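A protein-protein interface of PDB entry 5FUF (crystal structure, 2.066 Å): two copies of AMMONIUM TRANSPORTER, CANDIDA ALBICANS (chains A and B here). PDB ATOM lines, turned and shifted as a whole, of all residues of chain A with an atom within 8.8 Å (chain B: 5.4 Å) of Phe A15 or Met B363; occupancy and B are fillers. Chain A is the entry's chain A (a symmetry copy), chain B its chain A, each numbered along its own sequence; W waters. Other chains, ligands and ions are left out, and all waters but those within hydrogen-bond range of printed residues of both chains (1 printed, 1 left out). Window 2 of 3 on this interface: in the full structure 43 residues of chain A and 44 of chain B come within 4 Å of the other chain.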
ATOM      1  N   GLN A   4       7.114  31.501  24.690  1.00  0.00           N
ATOM      2  CA  GLN A   4       8.305  31.525  23.853  1.00  0.00           C
ATOM      3  C   GLN A   4       9.107  30.218  23.993  1.00  0.00           C
ATOM      4  O   GLN A   4      10.026  29.963  23.214  1.00  0.00           O
ATOM      5  CB  GLN A   4       9.167  32.733  24.203  1.00  0.00           C
ATOM      6  CG  GLN A   4       9.974  33.257  23.040  1.00  0.00           C
ATOM      7  CD  GLN A   4      10.508  34.648  23.296  1.00  0.00           C
ATOM      8  OE1 GLN A   4      10.400  35.177  24.407  1.00  0.00           O
ATOM      9  NE2 GLN A   4      11.083  35.257  22.266  1.00  0.00           N
ATOM     10  N   GLY A  12      13.125  26.392  21.538  1.00  0.00           N
ATOM     11  CA  GLY A  12      13.111  27.844  21.596  1.00  0.00           C
ATOM     12  C   GLY A  12      14.443  28.406  21.146  1.00  0.00           C
ATOM     13  O   GLY A  12      15.408  27.681  20.906  1.00  0.00           O
ATOM     14  N   ASP A  13      14.482  29.729  21.048  1.00  0.00           N
ATOM     15  CA  ASP A  13      15.657  30.458  20.580  1.00  0.00           C
ATOM     16  C   ASP A  13      16.563  30.775  21.766  1.00  0.00           C
ATOM     17  O   ASP A  13      16.164  31.519  22.672  1.00  0.00           O
ATOM     18  CB  ASP A  13      15.214  31.742  19.870  1.00  0.00           C
ATOM     19  CG  ASP A  13      16.353  32.473  19.175  1.00  0.00           C
ATOM     20  OD1 ASP A  13      17.543  32.163  19.413  1.00  0.00           O
ATOM     21  OD2 ASP A  13      16.044  33.390  18.384  1.00  0.00           O
ATOM     22  N   VAL A  14      17.793  30.239  21.746  1.00  0.00           N
ATOM     23  CA  VAL A  14      18.717  30.442  22.860  1.00  0.00           C
ATOM     24  C   VAL A  14      19.070  31.914  23.040  1.00  0.00           C
ATOM     25  O   VAL A  14      19.438  32.327  24.142  1.00  0.00           O
ATOM     26  CB  VAL A  14      20.003  29.586  22.697  1.00  0.00           C
ATOM     27  CG1 VAL A  14      19.681  28.079  22.847  1.00  0.00           C
ATOM     28  CG2 VAL A  14      20.703  29.873  21.354  1.00  0.00           C
ATOM     29  N   PHE A  15      18.973  32.721  21.981  1.00  0.00           N
ATOM     30  CA  PHE A  15      19.242  34.153  22.100  1.00  0.00           C
ATOM     31  C   PHE A  15      18.061  34.936  22.660  1.00  0.00           C
ATOM     32  O   PHE A  15      18.220  36.125  22.970  1.00  0.00           O
ATOM     33  CB  PHE A  15      19.652  34.735  20.740  1.00  0.00           C
ATOM     34  CG  PHE A  15      20.936  34.171  20.211  1.00  0.00           C
ATOM     35  CD1 PHE A  15      22.139  34.443  20.846  1.00  0.00           C
ATOM     36  CD2 PHE A  15      20.945  33.359  19.092  1.00  0.00           C
ATOM     37  CE1 PHE A  15      23.335  33.908  20.376  1.00  0.00           C
ATOM     38  CE2 PHE A  15      22.149  32.811  18.612  1.00  0.00           C
ATOM     39  CZ  PHE A  15      23.338  33.100  19.256  1.00  0.00           C
ATOM     40  N   LYS A  16      16.891  34.311  22.803  1.00  0.00           N
ATOM     41  CA  LYS A  16      15.722  34.992  23.357  1.00  0.00           C
ATOM     42  C   LYS A  16      15.258  34.433  24.692  1.00  0.00           C
ATOM     43  O   LYS A  16      14.705  35.184  25.496  1.00  0.00           O
ATOM     44  CB  LYS A  16      14.548  34.937  22.371  1.00  0.00           C
ATOM     45  CG  LYS A  16      14.803  35.646  21.047  1.00  0.00           C
ATOM     46  CD  LYS A  16      13.580  35.572  20.148  1.00  0.00           C
ATOM     47  CE  LYS A  16      13.874  36.123  18.763  1.00  0.00           C
ATOM     48  NZ  LYS A  16      12.647  36.271  17.941  1.00  0.00           N
ATOM     49  N   VAL A  17      15.463  33.136  24.951  1.00  0.00           N
ATOM     50  CA  VAL A  17      15.002  32.492  26.172  1.00  0.00           C
ATOM     51  C   VAL A  17      16.118  31.628  26.752  1.00  0.00           C
ATOM     52  O   VAL A  17      17.030  31.182  26.049  1.00  0.00           O
ATOM     53  CB  VAL A  17      13.733  31.631  25.946  1.00  0.00           C
ATOM     54  CG1 VAL A  17      12.574  32.480  25.423  1.00  0.00           C
ATOM     55  CG2 VAL A  17      14.025  30.466  25.004  1.00  0.00           C
ATOM     56  N   ASP A  18      16.020  31.398  28.059  1.00  0.00           N
ATOM     57  CA  ASP A  18      16.900  30.495  28.792  1.00  0.00           C
ATOM     58  C   ASP A  18      16.182  29.153  28.867  1.00  0.00           C
ATOM     59  O   ASP A  18      15.317  28.953  29.722  1.00  0.00           O
ATOM     60  CB  ASP A  18      17.224  31.057  30.175  1.00  0.00           C
ATOM     61  CG  ASP A  18      18.094  30.109  31.018  1.00  0.00           C
ATOM     62  OD1 ASP A  18      18.520  29.039  30.505  1.00  0.00           O
ATOM     63  OD2 ASP A  18      18.367  30.452  32.191  1.00  0.00           O
ATOM     64  N   LEU A  19      16.544  28.233  27.963  1.00  0.00           N
ATOM     65  CA  LEU A  19      15.885  26.927  27.904  1.00  0.00           C
ATOM     66  C   LEU A  19      15.998  26.152  29.212  1.00  0.00           C
ATOM     67  O   LEU A  19      15.189  25.250  29.452  1.00  0.00           O
ATOM     68  CB  LEU A  19      16.465  26.078  26.767  1.00  0.00           C
ATOM     69  CG  LEU A  19      16.262  26.616  25.342  1.00  0.00           C
ATOM     70  CD1 LEU A  19      17.048  25.752  24.343  1.00  0.00           C
ATOM     71  CD2 LEU A  19      14.778  26.636  24.993  1.00  0.00           C
ATOM     72  N   ASN A  20      16.973  26.481  30.057  1.00  0.00           N
ATOM     73  CA  ASN A  20      17.147  25.777  31.330  1.00  0.00           C
ATOM     74  C   ASN A  20      16.038  26.083  32.338  1.00  0.00           C
ATOM     75  O   ASN A  20      15.798  25.270  33.243  1.00  0.00           O
ATOM     76  CB  ASN A  20      18.521  26.122  31.913  1.00  0.00           C
ATOM     77  CG  ASN A  20      19.665  25.751  30.958  1.00  0.00           C
ATOM     78  OD1 ASN A  20      19.983  24.573  30.801  1.00  0.00           O
ATOM     79  ND2 ASN A  20      20.291  26.753  30.339  1.00  0.00           N
ATOM     80  N   LEU A 105      17.868  19.504  21.561  1.00  0.00           N
ATOM     81  CA  LEU A 105      18.414  20.462  22.515  1.00  0.00           C
ATOM     82  C   LEU A 105      17.532  20.616  23.754  1.00  0.00           C
ATOM     83  O   LEU A 105      17.544  19.759  24.643  1.00  0.00           O
ATOM     84  CB  LEU A 105      18.627  21.828  21.838  1.00  0.00           C
ATOM     85  CG  LEU A 105      19.387  22.912  22.631  1.00  0.00           C
ATOM     86  CD1 LEU A 105      20.741  22.407  23.080  1.00  0.00           C
ATOM     87  CD2 LEU A 105      19.533  24.215  21.838  1.00  0.00           C
ATOM     88  N   ARG B 250      24.070  22.885  28.765  1.00  0.00           N
ATOM     89  CA  ARG B 250      25.324  22.898  28.016  1.00  0.00           C
ATOM     90  C   ARG B 250      26.311  21.887  28.590  1.00  0.00           C
ATOM     91  O   ARG B 250      27.197  21.411  27.870  1.00  0.00           O
ATOM     92  CB  ARG B 250      25.962  24.284  28.001  1.00  0.00           C
ATOM     93  CG  ARG B 250      27.178  24.400  27.057  1.00  0.00           C
ATOM     94  CD  ARG B 250      27.584  25.864  26.800  1.00  0.00           C
ATOM     95  NE  ARG B 250      28.342  26.431  27.907  1.00  0.00           N
ATOM     96  CZ  ARG B 250      29.641  26.711  27.876  1.00  0.00           C
ATOM     97  NH1 ARG B 250      30.353  26.509  26.772  1.00  0.00           N
ATOM     98  NH2 ARG B 250      30.223  27.218  28.956  1.00  0.00           N
ATOM     99  N   ALA B 358      30.737  27.812  17.820  1.00  0.00           N
ATOM    100  CA  ALA B 358      29.489  28.453  17.422  1.00  0.00           C
ATOM    101  C   ALA B 358      28.889  29.213  18.599  1.00  0.00           C
ATOM    102  O   ALA B 358      28.703  28.642  19.680  1.00  0.00           O
ATOM    103  CB  ALA B 358      28.485  27.420  16.898  1.00  0.00           C
ATOM    104  N   ASP B 359      28.554  30.493  18.380  1.00  0.00           N
ATOM    105  CA  ASP B 359      28.023  31.307  19.476  1.00  0.00           C
ATOM    106  C   ASP B 359      26.703  30.760  20.003  1.00  0.00           C
ATOM    107  O   ASP B 359      26.437  30.861  21.205  1.00  0.00           O
ATOM    108  CB  ASP B 359      27.879  32.786  19.060  1.00  0.00           C
ATOM    109  CG  ASP B 359      27.010  32.999  17.817  1.00  0.00           C
ATOM    110  OD1 ASP B 359      26.399  32.042  17.292  1.00  0.00           O
ATOM    111  OD2 ASP B 359      26.953  34.162  17.355  1.00  0.00           O
ATOM    112  N   TYR B 360      25.885  30.133  19.151  1.00  0.00           N
ATOM    113  CA  TYR B 360      24.619  29.589  19.643  1.00  0.00           C
ATOM    114  C   TYR B 360      24.815  28.352  20.518  1.00  0.00           C
ATOM    115  O   TYR B 360      23.912  28.015  21.290  1.00  0.00           O
ATOM    116  CB  TYR B 360      23.663  29.272  18.479  1.00  0.00           C
ATOM    117  CG  TYR B 360      24.272  28.494  17.325  1.00  0.00           C
ATOM    118  CD1 TYR B 360      24.312  27.098  17.341  1.00  0.00           C
ATOM    119  CD2 TYR B 360      24.792  29.154  16.209  1.00  0.00           C
ATOM    120  CE1 TYR B 360      24.868  26.377  16.284  1.00  0.00           C
ATOM    121  CE2 TYR B 360      25.354  28.443  15.146  1.00  0.00           C
ATOM    122  CZ  TYR B 360      25.383  27.056  15.190  1.00  0.00           C
ATOM    123  OH  TYR B 360      25.936  26.348  14.143  1.00  0.00           O
ATOM    124  N   VAL B 361      25.969  27.677  20.437  1.00  0.00           N
ATOM    125  CA  VAL B 361      26.208  26.570  21.362  1.00  0.00           C
ATOM    126  C   VAL B 361      26.625  27.096  22.732  1.00  0.00           C
ATOM    127  O   VAL B 361      26.115  26.642  23.763  1.00  0.00           O
ATOM    128  CB  VAL B 361      27.248  25.587  20.794  1.00  0.00           C
ATOM    129  CG1 VAL B 361      27.661  24.571  21.870  1.00  0.00           C
ATOM    130  CG2 VAL B 361      26.699  24.872  19.551  1.00  0.00           C
ATOM    131  N   ALA B 362      27.567  28.043  22.768  1.00  0.00           N
ATOM    132  CA  ALA B 362      27.916  28.697  24.026  1.00  0.00           C
ATOM    133  C   ALA B 362      26.697  29.337  24.695  1.00  0.00           C
ATOM    134  O   ALA B 362      26.568  29.280  25.926  1.00  0.00           O
ATOM    135  CB  ALA B 362      29.002  29.754  23.782  1.00  0.00           C
ATOM    136  N   MET B 363      25.789  29.926  23.908  1.00  0.00           N
ATOM    137  CA  MET B 363      24.625  30.640  24.445  1.00  0.00           C
ATOM    138  C   MET B 363      23.618  29.709  25.120  1.00  0.00           C
ATOM    139  O   MET B 363      22.697  30.194  25.789  1.00  0.00           O
ATOM    140  CB  MET B 363      23.953  31.440  23.318  1.00  0.00           C
ATOM    141  CG  MET B 363      22.904  32.465  23.765  1.00  0.00           C
ATOM    142  SD  MET B 363      23.489  33.608  25.037  1.00  0.00           S
ATOM    143  CE  MET B 363      24.850  34.382  24.198  1.00  0.00           C
ATOM    144  N   ILE B 364      23.792  28.388  24.995  1.00  0.00           N
ATOM    145  CA  ILE B 364      22.907  27.435  25.667  1.00  0.00           C
ATOM    146  C   ILE B 364      22.805  27.725  27.162  1.00  0.00           C
ATOM    147  O   ILE B 364      21.745  27.528  27.767  1.00  0.00           O
ATOM    148  CB  ILE B 364      23.391  25.994  25.394  1.00  0.00           C
ATOM    149  CG1 ILE B 364      23.107  25.598  23.941  1.00  0.00           C
ATOM    150  CG2 ILE B 364      22.731  25.012  26.352  1.00  0.00           C
ATOM    151  CD1 ILE B 364      23.800  24.264  23.501  1.00  0.00           C
ATOM    152  N   ASP B 365      23.882  28.204  27.788  1.00  0.00           N
ATOM    153  CA  ASP B 365      23.801  28.624  29.183  1.00  0.00           C
ATOM    154  C   ASP B 365      24.076  30.116  29.351  1.00  0.00           C
ATOM    155  O   ASP B 365      24.474  30.551  30.434  1.00  0.00           O
ATOM    156  CB  ASP B 365      24.754  27.803  30.065  1.00  0.00           C
ATOM    157  CG  ASP B 365      26.221  27.989  29.692  1.00  0.00           C
ATOM    158  OD1 ASP B 365      26.525  28.796  28.788  1.00  0.00           O
ATOM    159  OD2 ASP B 365      27.084  27.331  30.330  1.00  0.00           O
ATOM    160  N   GLY B 366      23.890  30.907  28.294  1.00  0.00           N
ATOM    161  CA  GLY B 366      24.126  32.338  28.369  1.00  0.00           C
ATOM    162  C   GLY B 366      25.573  32.767  28.213  1.00  0.00           C
ATOM    163  O   GLY B 366      25.856  33.962  28.338  1.00  0.00           O
ATOM    164  N   THR B 367      26.499  31.841  27.942  1.00  0.00           N
ATOM    165  CA  THR B 367      27.886  32.221  27.698  1.00  0.00           C
ATOM    166  C   THR B 367      27.989  32.959  26.370  1.00  0.00           C
ATOM    167  O   THR B 367      27.422  32.522  25.363  1.00  0.00           O
ATOM    168  CB  THR B 367      28.797  30.984  27.686  1.00  0.00           C
ATOM    169  OG1 THR B 367      28.654  30.254  28.912  1.00  0.00           O
ATOM    170  CG2 THR B 367      30.276  31.375  27.501  1.00  0.00           C
ATOM    171  N   GLU B 368      28.707  34.084  26.364  1.00  0.00           N
ATOM    172  CA  GLU B 368      28.831  34.942  25.188  1.00  0.00           C
ATOM    173  C   GLU B 368      30.220  34.803  24.578  1.00  0.00           C
ATOM    174  O   GLU B 368      31.227  35.058  25.247  1.00  0.00           O
ATOM    175  CB  GLU B 368      28.553  36.403  25.550  1.00  0.00           C
ATOM    176  CG  GLU B 368      27.075  36.690  25.738  1.00  0.00           C
ATOM    177  CD  GLU B 368      26.808  38.040  26.376  1.00  0.00           C
ATOM    178  OE1 GLU B 368      27.782  38.758  26.694  1.00  0.00           O
ATOM    179  OE2 GLU B 368      25.619  38.378  26.563  1.00  0.00           O
HETATM  180  O   HOH W   1      19.135  28.335  26.696  1.00  0.00           O
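O of Ile B364 sits at hydrogen-bond distance from ND2 of Asn A20, at 3.1 Å.
The side-chain carboxylate of Asp A13 sits at hydrogen-bond distance from the backbone NH of Phe A15 (3.0 Å). The side-chain carboxylate (OD1) of Asp A18 lies within hydrogen-bond range of the side-chain amide nitrogen (ND2) of Asn A20, at 2.9 Å.
Among the printed residues, merely in contact across the chains: Val A14 with Tyr B360 (3.7 Å), Val A14 with Met B363 (3.5 Å), Phe A15 with Asp B359 (3.8 Å), Phe A15 with Tyr B360 (3.8 Å), Phe A15 with Met B363 (3.6 Å) and Leu A105 with Ile B364 (3.6 Å).
Phe A15 touches just these residues of chain B: Asp B359, Tyr B360 and Met B363. Asp A18 touches none of the printed residues of chain B. Of the printed residues of chain B, Asn A20 touches Ile B364. Of the printed residues of chain B, Leu A105 touches Ile B364. Of the printed residues of chain A, Asp B359 touches Phe A15 (3.8 Å). No residue of chain A comes within 4 Å of Ala B362. Met B363 touches just these residues of chain A: Val A14 and Phe A15. Printed residues of chain A within 4 Å of Ile B364: Asn A20 and Leu A105. No residue of chain A comes within 4 Å of Gly B366. The nearest printed residue of chain B that does not touch Leu A105 is Tyr B360 (5.8 Å).
Hydrophobic or aromatic side chains of chain B within 4 Å of the printed part of chain A: Tyr B360, Met B363 and Ile B364. Of the 11 printed residues of chain A, 4 touch a printed residue of chain B. Among the printed residues, 7 pairs touch across the chains.
No position is printed for both chains. Of the 7 pairs that touch across the chains among the printed residues, none has its exchanged pair printed and touching as well.
Water W1 lies within hydrogen-bond range of N of Leu A19 (2.9 Å) and O of Ile B364 (2.9 Å).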
